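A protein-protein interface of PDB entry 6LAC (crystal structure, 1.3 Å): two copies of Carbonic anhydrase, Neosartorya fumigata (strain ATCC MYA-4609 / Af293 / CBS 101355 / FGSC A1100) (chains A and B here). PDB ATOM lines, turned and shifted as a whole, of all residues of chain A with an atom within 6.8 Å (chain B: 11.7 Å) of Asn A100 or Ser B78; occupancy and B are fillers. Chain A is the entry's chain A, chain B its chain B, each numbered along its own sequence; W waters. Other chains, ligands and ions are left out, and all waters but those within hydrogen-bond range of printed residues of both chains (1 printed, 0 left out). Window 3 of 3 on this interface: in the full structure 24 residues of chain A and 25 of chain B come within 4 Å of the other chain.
CG1 of Ile A94 touches OH of Tyr B74 (3.6 Å).
CE1 of Tyr B74 touches ND2 of Asn A100, at 3.998 Å.
OG of Ser B78 touches ND2 of Asn A100, at 3.6 Å.
Gly A102 touches Tyr B74 (O to CA, 3.6 Å).
O of Lys B69 touches NE2 of Gln A104, at 3.8 Å.
Gln A104 touches Ala B70 (OE1 to CA, 3.5 Å).
The backbone NH of Gly A102 is in hydrogen-bond range of the side-chain amide oxygen of Asn A100, 3.0 Å away.
The backbone carbonyl oxygen (O) of Tyr B74 lies within hydrogen-bond range of the backbone NH (N) of Leu B79, 3.2 Å away.
Of the 25 printed residues of chain B, 4 touch a printed residue of chain A.
Hydrophobic or aromatic side chains of chain B that line the printed part of chain A: Ala B70 and Tyr B74.
No position is printed for both chains.
Of the printed residues of chain B, Asn A100 touches Tyr B74 and Ser B78.
No residue of chain B comes within 4 Å of Val A99.
No residue of chain B comes within 4 Å of Ser A108.
Of the printed residues of chain B, Ile A94 touches Tyr B74 (3.6 Å).
Printed residues of chain A within 4 Å of Lys B69: Gln A104.
Printed residues of chain A within 4 Å of Tyr B74: Ile A94, Asn A100 and Gly A102.
Printed residues of chain A within 4 Å of Ala B70: Gln A104.
Leu B79 touches none of the printed residues of chain A.
The nearest printed residue of chain A that does not touch Ala B70 is Gly A102 (5.0 Å).
Water W1 lies within hydrogen-bond range of O of Ala B70 (2.8 Å), O of Gly A102 (2.9 Å) and N of Gln A104 (3.0 Å).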
ATOM      1  N   HIS A  93     -13.036 -13.709   9.768  1.00  0.00           N
ATOM      2  CA  HIS A  93     -14.100 -13.948  10.757  1.00  0.00           C
ATOM      3  C   HIS A  93     -14.206 -15.423  11.053  1.00  0.00           C
ATOM      4  O   HIS A  93     -14.688 -15.844  12.128  1.00  0.00           O
ATOM      5  CB  HIS A  93     -15.441 -13.360  10.297  1.00  0.00           C
ATOM      6  CG  HIS A  93     -15.384 -11.894  10.139  1.00  0.00           C
ATOM      7  ND1 HIS A  93     -15.526 -11.005  11.182  1.00  0.00           N
ATOM      8  CD2 HIS A  93     -15.144 -11.144   9.051  1.00  0.00           C
ATOM      9  CE1 HIS A  93     -15.388  -9.769  10.728  1.00  0.00           C
ATOM     10  NE2 HIS A  93     -15.154  -9.826   9.436  1.00  0.00           N
ATOM     11  N   ILE A  94     -13.696 -16.283  10.177  1.00  0.00           N
ATOM     12  CA  ILE A  94     -13.793 -17.735  10.386  1.00  0.00           C
ATOM     13  C   ILE A  94     -12.641 -18.159  11.305  1.00  0.00           C
ATOM     14  O   ILE A  94     -12.910 -18.836  12.355  1.00  0.00           O
ATOM     15  CB  ILE A  94     -13.876 -18.448   9.020  1.00  0.00           C
ATOM     16  CG1 ILE A  94     -15.167 -18.092   8.285  1.00  0.00           C
ATOM     17  CG2 ILE A  94     -13.719 -19.936   9.191  1.00  0.00           C
ATOM     18  CD1 ILE A  94     -15.132 -18.450   6.836  1.00  0.00           C
ATOM     19  N   SER A  96     -10.929 -17.049  13.828  1.00  0.00           N
ATOM     20  CA  SER A  96     -10.970 -15.926  14.792  1.00  0.00           C
ATOM     21  C   SER A  96     -11.694 -16.387  16.040  1.00  0.00           C
ATOM     22  O   SER A  96     -12.451 -17.357  15.997  1.00  0.00           O
ATOM     23  CB  SER A  96     -11.587 -14.657  14.256  1.00  0.00           C
ATOM     24  OG  SER A  96     -12.981 -14.583  14.484  1.00  0.00           O
ATOM     25  N   GLY A  97     -11.438 -15.659  17.119  1.00  0.00           N
ATOM     26  CA  GLY A  97     -12.156 -15.812  18.394  1.00  0.00           C
ATOM     27  C   GLY A  97     -12.013 -17.197  18.965  1.00  0.00           C
ATOM     28  O   GLY A  97     -10.981 -17.889  18.692  1.00  0.00           O
ATOM     29  N   GLU A  98     -13.030 -17.614  19.729  1.00  0.00           N
ATOM     30  CA  GLU A  98     -13.003 -18.835  20.580  1.00  0.00           C
ATOM     31  C   GLU A  98     -14.131 -19.790  20.177  1.00  0.00           C
ATOM     32  O   GLU A  98     -14.031 -20.954  20.565  1.00  0.00           O
ATOM     33  CB  GLU A  98     -13.087 -18.446  22.061  1.00  0.00           C
ATOM     34  CG  GLU A  98     -11.878 -17.678  22.560  1.00  0.00           C
ATOM     35  CD  GLU A  98     -10.589 -18.487  22.585  1.00  0.00           C
ATOM     36  OE1 GLU A  98     -10.661 -19.745  22.516  1.00  0.00           O
ATOM     37  OE2 GLU A  98      -9.515 -17.861  22.670  1.00  0.00           O
ATOM     38  N   VAL A  99     -15.134 -19.324  19.418  1.00  0.00           N
ATOM     39  CA  VAL A  99     -16.338 -20.103  18.982  1.00  0.00           C
ATOM     40  C   VAL A  99     -16.980 -19.406  17.776  1.00  0.00           C
ATOM     41  O   VAL A  99     -16.807 -18.181  17.680  1.00  0.00           O
ATOM     42  CB  VAL A  99     -17.386 -20.236  20.109  1.00  0.00           C
ATOM     43  CG1 VAL A  99     -18.128 -21.561  20.029  1.00  0.00           C
ATOM     44  CG2 VAL A  99     -16.814 -20.024  21.505  1.00  0.00           C
ATOM     45  N   ASN A 100     -17.687 -20.161  16.911  1.00  0.00           N
ATOM     46  CA  ASN A 100     -18.750 -19.664  15.982  1.00  0.00           C
ATOM     47  C   ASN A 100     -19.753 -20.789  15.666  1.00  0.00           C
ATOM     48  O   ASN A 100     -19.361 -21.749  14.959  1.00  0.00           O
ATOM     49  CB  ASN A 100     -18.195 -19.088  14.673  1.00  0.00           C
ATOM     50  CG  ASN A 100     -19.273 -18.439  13.823  1.00  0.00           C
ATOM     51  OD1 ASN A 100     -20.322 -19.030  13.579  1.00  0.00           O
ATOM     52  ND2 ASN A 100     -19.047 -17.210  13.389  1.00  0.00           N
ATOM     53  N   ALA A 101     -21.012 -20.647  16.113  1.00  0.00           N
ATOM     54  CA  ALA A 101     -22.059 -21.705  16.117  1.00  0.00           C
ATOM     55  C   ALA A 101     -22.467 -22.107  14.692  1.00  0.00           C
ATOM     56  O   ALA A 101     -22.812 -23.288  14.485  1.00  0.00           O
ATOM     57  CB  ALA A 101     -23.264 -21.243  16.902  1.00  0.00           C
ATOM     58  N   GLY A 102     -22.416 -21.176  13.732  1.00  0.00           N
ATOM     59  CA  GLY A 102     -22.877 -21.420  12.347  1.00  0.00           C
ATOM     60  C   GLY A 102     -21.822 -22.117  11.501  1.00  0.00           C
ATOM     61  O   GLY A 102     -22.153 -22.433  10.341  1.00  0.00           O
ATOM     62  N   LEU A 103     -20.627 -22.345  12.049  1.00  0.00           N
ATOM     63  CA  LEU A 103     -19.525 -23.100  11.386  1.00  0.00           C
ATOM     64  C   LEU A 103     -19.640 -24.583  11.755  1.00  0.00           C
ATOM     65  O   LEU A 103     -19.521 -24.913  12.931  1.00  0.00           O
ATOM     66  CB  LEU A 103     -18.177 -22.495  11.799  1.00  0.00           C
ATOM     67  CG  LEU A 103     -16.971 -22.959  10.984  1.00  0.00           C
ATOM     68  CD1 LEU A 103     -17.059 -22.504   9.532  1.00  0.00           C
ATOM     69  CD2 LEU A 103     -15.678 -22.491  11.628  1.00  0.00           C
ATOM     70  N   GLN A 104     -19.849 -25.456  10.768  1.00  0.00           N
ATOM     71  CA  GLN A 104     -20.025 -26.912  10.964  1.00  0.00           C
ATOM     72  C   GLN A 104     -18.668 -27.634  10.996  1.00  0.00           C
ATOM     73  O   GLN A 104     -17.631 -27.041  10.597  1.00  0.00           O
ATOM     74  CB  GLN A 104     -20.891 -27.487   9.849  1.00  0.00           C
ATOM     75  CG  GLN A 104     -22.234 -26.767   9.753  1.00  0.00           C
ATOM     76  CD  GLN A 104     -23.000 -27.081   8.492  1.00  0.00           C
ATOM     77  OE1 GLN A 104     -22.667 -28.007   7.760  1.00  0.00           O
ATOM     78  NE2 GLN A 104     -24.069 -26.322   8.260  1.00  0.00           N
ATOM     79  N   SER A 108     -15.070 -26.526  12.153  1.00  0.00           N
ATOM     80  CA  SER A 108     -15.097 -26.110  13.571  1.00  0.00           C
ATOM     81  C   SER A 108     -14.143 -26.983  14.388  1.00  0.00           C
ATOM     82  O   SER A 108     -13.524 -26.426  15.260  1.00  0.00           O
ATOM     83  CB  SER A 108     -16.496 -26.151  14.087  1.00  0.00           C
ATOM     84  OG  SER A 108     -16.958 -27.474  14.064  1.00  0.00           O
ATOM     85  N   ARG A 115      -6.835 -24.153  18.503  1.00  0.00           N
ATOM     86  CA  ARG A 115      -6.920 -23.385  19.757  1.00  0.00           C
ATOM     87  C   ARG A 115      -6.349 -24.221  20.900  1.00  0.00           C
ATOM     88  O   ARG A 115      -5.724 -23.637  21.771  1.00  0.00           O
ATOM     89  CB  ARG A 115      -8.356 -22.926  20.010  1.00  0.00           C
ATOM     90  CG  ARG A 115      -8.813 -21.848  19.029  1.00  0.00           C
ATOM     91  CD  ARG A 115     -10.076 -21.063  19.351  1.00  0.00           C
ATOM     92  NE  ARG A 115     -11.157 -21.791  18.752  1.00  0.00           N
ATOM     93  CZ  ARG A 115     -11.938 -21.467  17.712  1.00  0.00           C
ATOM     94  NH1 ARG A 115     -11.835 -20.267  17.140  1.00  0.00           N
ATOM     95  NH2 ARG A 115     -12.838 -22.330  17.242  1.00  0.00           N
ATOM     96  N   GLY B  26     -24.087  -2.673   1.675  1.00  0.00           N
ATOM     97  CA  GLY B  26     -23.635  -2.993   3.038  1.00  0.00           C
ATOM     98  C   GLY B  26     -24.015  -4.389   3.465  1.00  0.00           C
ATOM     99  O   GLY B  26     -23.748  -4.723   4.596  1.00  0.00           O
ATOM    100  N   GLN B  27     -24.549  -5.210   2.564  1.00  0.00           N
ATOM    101  CA  GLN B  27     -24.919  -6.607   2.917  1.00  0.00           C
ATOM    102  C   GLN B  27     -23.895  -7.556   2.284  1.00  0.00           C
ATOM    103  O   GLN B  27     -23.190  -7.142   1.358  1.00  0.00           O
ATOM    104  CB  GLN B  27     -26.327  -6.973   2.432  1.00  0.00           C
ATOM    105  CG  GLN B  27     -27.320  -5.819   2.464  1.00  0.00           C
ATOM    106  CD  GLN B  27     -27.413  -5.268   3.856  1.00  0.00           C
ATOM    107  OE1 GLN B  27     -27.196  -4.073   4.076  1.00  0.00           O
ATOM    108  NE2 GLN B  27     -27.662  -6.161   4.800  1.00  0.00           N
ATOM    109  N   GLN B  28     -23.777  -8.767   2.769  1.00  0.00           N
ATOM    110  CA  GLN B  28     -22.892  -9.757   2.086  1.00  0.00           C
ATOM    111  C   GLN B  28     -23.707 -10.626   1.145  1.00  0.00           C
ATOM    112  O   GLN B  28     -24.904 -10.879   1.355  1.00  0.00           O
ATOM    113  CB  GLN B  28     -22.137 -10.625   3.045  1.00  0.00           C
ATOM    114  CG  GLN B  28     -21.008  -9.817   3.624  1.00  0.00           C
ATOM    115  CD  GLN B  28     -20.474 -10.610   4.752  1.00  0.00           C
ATOM    116  OE1 GLN B  28     -21.152 -10.753   5.774  1.00  0.00           O
ATOM    117  NE2 GLN B  28     -19.356 -11.254   4.486  1.00  0.00           N
ATOM    118  N   VAL B  29     -23.127 -10.913   0.022  1.00  0.00           N
ATOM    119  CA  VAL B  29     -23.718 -11.752  -1.050  1.00  0.00           C
ATOM    120  C   VAL B  29     -22.829 -12.987  -1.217  1.00  0.00           C
ATOM    121  O   VAL B  29     -21.592 -12.844  -1.321  1.00  0.00           O
ATOM    122  CB  VAL B  29     -23.788 -10.963  -2.347  1.00  0.00           C
ATOM    123  CG1 VAL B  29     -24.197 -11.842  -3.511  1.00  0.00           C
ATOM    124  CG2 VAL B  29     -24.655  -9.722  -2.228  1.00  0.00           C
ATOM    125  N   LEU B  30     -23.422 -14.166  -1.228  1.00  0.00           N
ATOM    126  CA  LEU B  30     -22.640 -15.386  -1.508  1.00  0.00           C
ATOM    127  C   LEU B  30     -22.471 -15.500  -3.014  1.00  0.00           C
ATOM    128  O   LEU B  30     -23.484 -15.577  -3.750  1.00  0.00           O
ATOM    129  CB  LEU B  30     -23.371 -16.605  -0.943  1.00  0.00           C
ATOM    130  CG  LEU B  30     -22.863 -17.968  -1.390  1.00  0.00           C
ATOM    131  CD1 LEU B  30     -21.376 -18.197  -1.032  1.00  0.00           C
ATOM    132  CD2 LEU B  30     -23.702 -19.088  -0.758  1.00  0.00           C
ATOM    133  N   PHE B  53     -18.878 -12.615  -0.350  1.00  0.00           N
ATOM    134  CA  PHE B  53     -18.513 -13.837   0.386  1.00  0.00           C
ATOM    135  C   PHE B  53     -18.390 -14.892  -0.701  1.00  0.00           C
ATOM    136  O   PHE B  53     -19.384 -15.283  -1.289  1.00  0.00           O
ATOM    137  CB  PHE B  53     -19.549 -14.157   1.447  1.00  0.00           C
ATOM    138  CG  PHE B  53     -19.180 -15.349   2.264  1.00  0.00           C
ATOM    139  CD1 PHE B  53     -18.231 -15.254   3.255  1.00  0.00           C
ATOM    140  CD2 PHE B  53     -19.807 -16.552   2.076  1.00  0.00           C
ATOM    141  CE1 PHE B  53     -17.886 -16.355   4.007  1.00  0.00           C
ATOM    142  CE2 PHE B  53     -19.457 -17.662   2.802  1.00  0.00           C
ATOM    143  CZ  PHE B  53     -18.520 -17.543   3.796  1.00  0.00           C
ATOM    144  N   LYS B  69     -22.848 -27.801   1.821  1.00  0.00           N
ATOM    145  CA  LYS B  69     -23.739 -27.662   2.977  1.00  0.00           C
ATOM    146  C   LYS B  69     -23.171 -26.658   3.961  1.00  0.00           C
ATOM    147  O   LYS B  69     -23.922 -25.829   4.493  1.00  0.00           O
ATOM    148  CB  LYS B  69     -23.968 -29.010   3.664  1.00  0.00           C
ATOM    149  CG  LYS B  69     -24.841 -29.956   2.845  1.00  0.00           C
ATOM    150  CD  LYS B  69     -26.177 -29.340   2.407  1.00  0.00           C
ATOM    151  CE  LYS B  69     -27.015 -30.222   1.505  1.00  0.00           C
ATOM    152  NZ  LYS B  69     -28.180 -29.500   0.929  1.00  0.00           N
ATOM    153  N   ALA B  70     -21.883 -26.798   4.266  1.00  0.00           N
ATOM    154  CA  ALA B  70     -21.273 -25.970   5.320  1.00  0.00           C
ATOM    155  C   ALA B  70     -21.216 -24.520   4.820  1.00  0.00           C
ATOM    156  O   ALA B  70     -21.414 -23.606   5.573  1.00  0.00           O
ATOM    157  CB  ALA B  70     -19.912 -26.472   5.705  1.00  0.00           C
ATOM    158  N   THR B  71     -20.863 -24.320   3.552  1.00  0.00           N
ATOM    159  CA  THR B  71     -20.708 -22.944   3.015  1.00  0.00           C
ATOM    160  C   THR B  71     -22.088 -22.285   2.955  1.00  0.00           C
ATOM    161  O   THR B  71     -22.240 -21.182   3.368  1.00  0.00           O
ATOM    162  CB  THR B  71     -19.972 -23.002   1.673  1.00  0.00           C
ATOM    163  OG1 THR B  71     -18.703 -23.643   1.842  1.00  0.00           O
ATOM    164  CG2 THR B  71     -19.823 -21.612   1.105  1.00  0.00           C
ATOM    165  N   LEU B  72     -23.065 -23.021   2.400  1.00  0.00           N
ATOM    166  CA  LEU B  72     -24.428 -22.454   2.320  1.00  0.00           C
ATOM    167  C   LEU B  72     -24.963 -22.197   3.737  1.00  0.00           C
ATOM    168  O   LEU B  72     -25.474 -21.120   4.056  1.00  0.00           O
ATOM    169  CB  LEU B  72     -25.291 -23.427   1.526  1.00  0.00           C
ATOM    170  CG  LEU B  72     -26.744 -22.987   1.382  1.00  0.00           C
ATOM    171  CD1 LEU B  72     -26.831 -21.705   0.579  1.00  0.00           C
ATOM    172  CD2 LEU B  72     -27.528 -24.097   0.743  1.00  0.00           C
ATOM    173  N   GLY B  73     -24.753 -23.143   4.651  1.00  0.00           N
ATOM    174  CA  GLY B  73     -25.217 -23.042   6.031  1.00  0.00           C
ATOM    175  C   GLY B  73     -24.596 -21.877   6.757  1.00  0.00           C
ATOM    176  O   GLY B  73     -25.318 -21.111   7.438  1.00  0.00           O
ATOM    177  N   TYR B  74     -23.272 -21.698   6.651  1.00  0.00           N
ATOM    178  CA  TYR B  74     -22.596 -20.551   7.289  1.00  0.00           C
ATOM    179  C   TYR B  74     -23.139 -19.235   6.704  1.00  0.00           C
ATOM    180  O   TYR B  74     -23.390 -18.272   7.426  1.00  0.00           O
ATOM    181  CB  TYR B  74     -21.072 -20.670   7.131  1.00  0.00           C
ATOM    182  CG  TYR B  74     -20.269 -19.557   7.712  1.00  0.00           C
ATOM    183  CD1 TYR B  74     -19.970 -19.535   9.053  1.00  0.00           C
ATOM    184  CD2 TYR B  74     -19.837 -18.483   6.964  1.00  0.00           C
ATOM    185  CE1 TYR B  74     -19.268 -18.487   9.607  1.00  0.00           C
ATOM    186  CE2 TYR B  74     -19.119 -17.432   7.492  1.00  0.00           C
ATOM    187  CZ  TYR B  74     -18.825 -17.433   8.844  1.00  0.00           C
ATOM    188  OH  TYR B  74     -18.138 -16.391   9.340  1.00  0.00           O
ATOM    189  N   ALA B  75     -23.249 -19.139   5.374  1.00  0.00           N
ATOM    190  CA  ALA B  75     -23.769 -17.933   4.688  1.00  0.00           C
ATOM    191  C   ALA B  75     -25.171 -17.539   5.217  1.00  0.00           C
ATOM    192  O   ALA B  75     -25.368 -16.396   5.551  1.00  0.00           O
ATOM    193  CB  ALA B  75     -23.770 -18.187   3.197  1.00  0.00           C
ATOM    194  N   LEU B  76     -26.056 -18.507   5.294  1.00  0.00           N
ATOM    195  CA  LEU B  76     -27.466 -18.213   5.709  1.00  0.00           C
ATOM    196  C   LEU B  76     -27.527 -17.978   7.226  1.00  0.00           C
ATOM    197  O   LEU B  76     -28.144 -16.971   7.624  1.00  0.00           O
ATOM    198  CB  LEU B  76     -28.358 -19.358   5.259  1.00  0.00           C
ATOM    199  CG  LEU B  76     -28.477 -19.643   3.771  1.00  0.00           C
ATOM    200  CD1 LEU B  76     -29.330 -20.868   3.529  1.00  0.00           C
ATOM    201  CD2 LEU B  76     -29.004 -18.453   2.959  1.00  0.00           C
ATOM    202  N   ASP B  77     -26.873 -18.801   8.057  1.00  0.00           N
ATOM    203  CA  ASP B  77     -27.070 -18.815   9.543  1.00  0.00           C
ATOM    204  C   ASP B  77     -26.224 -17.729  10.196  1.00  0.00           C
ATOM    205  O   ASP B  77     -26.765 -16.948  11.000  1.00  0.00           O
ATOM    206  CB  ASP B  77     -26.670 -20.148  10.182  1.00  0.00           C
ATOM    207  CG  ASP B  77     -27.532 -21.322   9.767  1.00  0.00           C
ATOM    208  OD1 ASP B  77     -28.515 -21.098   9.046  1.00  0.00           O
ATOM    209  OD2 ASP B  77     -27.199 -22.458  10.157  1.00  0.00           O
ATOM    210  N   SER B  78     -24.922 -17.704   9.923  1.00  0.00           N
ATOM    211  CA  SER B  78     -23.961 -16.767  10.548  1.00  0.00           C
ATOM    212  C   SER B  78     -23.993 -15.409   9.866  1.00  0.00           C
ATOM    213  O   SER B  78     -24.029 -14.369  10.574  1.00  0.00           O
ATOM    214  CB  SER B  78     -22.579 -17.368  10.578  1.00  0.00           C
ATOM    215  OG  SER B  78     -21.617 -16.405  10.949  1.00  0.00           O
ATOM    216  N   LEU B  79     -24.010 -15.357   8.537  1.00  0.00           N
ATOM    217  CA  LEU B  79     -23.862 -14.070   7.856  1.00  0.00           C
ATOM    218  C   LEU B  79     -25.256 -13.481   7.521  1.00  0.00           C
ATOM    219  O   LEU B  79     -25.281 -12.368   7.078  1.00  0.00           O
ATOM    220  CB  LEU B  79     -23.014 -14.297   6.608  1.00  0.00           C
ATOM    221  CG  LEU B  79     -21.583 -14.789   6.871  1.00  0.00           C
ATOM    222  CD1 LEU B  79     -20.795 -14.746   5.582  1.00  0.00           C
ATOM    223  CD2 LEU B  79     -20.885 -13.938   7.938  1.00  0.00           C
ATOM    224  N   LYS B  80     -26.274 -14.289   7.629  1.00  0.00           N
ATOM    225  CA  LYS B  80     -27.670 -13.817   7.393  1.00  0.00           C
ATOM    226  C   LYS B  80     -27.769 -13.328   5.939  1.00  0.00           C
ATOM    227  O   LYS B  80     -28.387 -12.279   5.642  1.00  0.00           O
ATOM    228  CB  LYS B  80     -28.068 -12.684   8.365  1.00  0.00           C
ATOM    229  CG  LYS B  80     -27.842 -12.996   9.848  1.00  0.00           C
ATOM    230  CD  LYS B  80     -28.973 -12.647  10.788  1.00  0.00           C
ATOM    231  CE  LYS B  80     -28.901 -13.436  12.084  1.00  0.00           C
ATOM    232  NZ  LYS B  80     -27.956 -12.823  13.044  1.00  0.00           N
ATOM    233  N   ILE B  81     -27.097 -14.015   5.009  1.00  0.00           N
ATOM    234  CA  ILE B  81     -27.064 -13.619   3.580  1.00  0.00           C
ATOM    235  C   ILE B  81     -28.425 -13.863   2.939  1.00  0.00           C
ATOM    236  O   ILE B  81     -28.927 -15.015   3.049  1.00  0.00           O
ATOM    237  CB  ILE B  81     -25.914 -14.370   2.860  1.00  0.00           C
ATOM    238  CG1 ILE B  81     -24.584 -13.797   3.318  1.00  0.00           C
ATOM    239  CG2 ILE B  81     -26.027 -14.303   1.353  1.00  0.00           C
ATOM    240  CD1 ILE B  81     -23.281 -14.371   2.729  1.00  0.00           C
ATOM    241  N   ARG B  82     -28.859 -12.871   2.179  1.00  0.00           N
ATOM    242  CA  ARG B  82     -30.198 -12.866   1.545  1.00  0.00           C
ATOM    243  C   ARG B  82     -30.100 -12.966   0.033  1.00  0.00           C
ATOM    244  O   ARG B  82     -31.141 -13.046  -0.634  1.00  0.00           O
ATOM    245  CB  ARG B  82     -30.970 -11.585   1.901  1.00  0.00           C
ATOM    246  CG  ARG B  82     -31.211 -11.365   3.392  1.00  0.00           C
ATOM    247  CD  ARG B  82     -32.682 -11.410   3.786  1.00  0.00           C
ATOM    248  NE  ARG B  82     -32.838 -11.500   5.229  1.00  0.00           N
ATOM    249  CZ  ARG B  82     -33.885 -11.032   5.909  1.00  0.00           C
ATOM    250  NH1 ARG B  82     -34.879 -10.415   5.288  1.00  0.00           N
ATOM    251  NH2 ARG B  82     -33.928 -11.177   7.219  1.00  0.00           N
ATOM    252  N   GLU B 151     -31.896 -25.780   3.247  1.00  0.00           N
ATOM    253  CA  GLU B 151     -31.724 -24.487   3.944  1.00  0.00           C
ATOM    254  C   GLU B 151     -32.140 -23.365   2.999  1.00  0.00           C
ATOM    255  O   GLU B 151     -32.741 -22.364   3.473  1.00  0.00           O
ATOM    256  CB  GLU B 151     -30.315 -24.303   4.488  1.00  0.00           C
ATOM    257  CG  GLU B 151     -30.101 -24.956   5.843  1.00  0.00           C
ATOM    258  CD  GLU B 151     -28.934 -24.389   6.644  1.00  0.00           C
ATOM    259  OE1 GLU B 151     -27.964 -25.153   6.895  1.00  0.00           O
ATOM    260  OE2 GLU B 151     -29.011 -23.190   7.053  1.00  0.00           O
ATOM    261  N   GLU B 154     -36.101 -23.261   2.811  1.00  0.00           N
ATOM    262  CA  GLU B 154     -36.693 -22.709   4.053  1.00  0.00           C
ATOM    263  C   GLU B 154     -36.638 -21.191   3.950  1.00  0.00           C
ATOM    264  O   GLU B 154     -37.655 -20.492   4.179  1.00  0.00           O
ATOM    265  CB  GLU B 154     -35.910 -23.203   5.254  1.00  0.00           C
ATOM    266  CG  GLU B 154     -36.368 -22.630   6.580  1.00  0.00           C
ATOM    267  CD  GLU B 154     -35.527 -23.041   7.778  1.00  0.00           C
ATOM    268  OE1 GLU B 154     -34.332 -23.413   7.596  1.00  0.00           O
ATOM    269  OE2 GLU B 154     -36.056 -22.962   8.915  1.00  0.00           O
ATOM    270  N   ALA B 155     -35.505 -20.637   3.529  1.00  0.00           N
ATOM    271  CA  ALA B 155     -35.352 -19.165   3.425  1.00  0.00           C
ATOM    272  C   ALA B 155     -36.208 -18.588   2.297  1.00  0.00           C
ATOM    273  O   ALA B 155     -36.830 -17.510   2.455  1.00  0.00           O
ATOM    274  CB  ALA B 155     -33.912 -18.824   3.230  1.00  0.00           C
ATOM    275  N   GLN B 160     -36.819 -14.625   2.257  1.00  0.00           N
ATOM    276  CA  GLN B 160     -35.566 -14.118   2.861  1.00  0.00           C
ATOM    277  C   GLN B 160     -34.373 -14.561   2.012  1.00  0.00           C
ATOM    278  O   GLN B 160     -33.288 -14.524   2.527  1.00  0.00           O
ATOM    279  CB  GLN B 160     -35.471 -14.614   4.301  1.00  0.00           C
ATOM    280  CG  GLN B 160     -36.424 -13.878   5.243  1.00  0.00           C
ATOM    281  CD  GLN B 160     -36.348 -14.343   6.676  1.00  0.00           C
ATOM    282  OE1 GLN B 160     -35.637 -15.242   7.024  1.00  0.00           O
ATOM    283  NE2 GLN B 160     -37.153 -13.749   7.514  1.00  0.00           N
ATOM    284  N   LEU B 161     -34.592 -14.990   0.783  1.00  0.00           N
ATOM    285  CA  LEU B 161     -33.435 -15.399  -0.054  1.00  0.00           C
ATOM    286  C   LEU B 161     -33.820 -15.278  -1.517  1.00  0.00           C
ATOM    287  O   LEU B 161     -34.933 -15.565  -1.852  1.00  0.00           O
ATOM    288  CB  LEU B 161     -33.081 -16.859   0.261  1.00  0.00           C
ATOM    289  CG  LEU B 161     -31.893 -17.443  -0.515  1.00  0.00           C
ATOM    290  CD1 LEU B 161     -30.610 -16.675  -0.215  1.00  0.00           C
ATOM    291  CD2 LEU B 161     -31.724 -18.917  -0.155  1.00  0.00           C
HETATM  292  O   HOH W   1     -20.968 -24.136   8.319  1.00  0.00           O
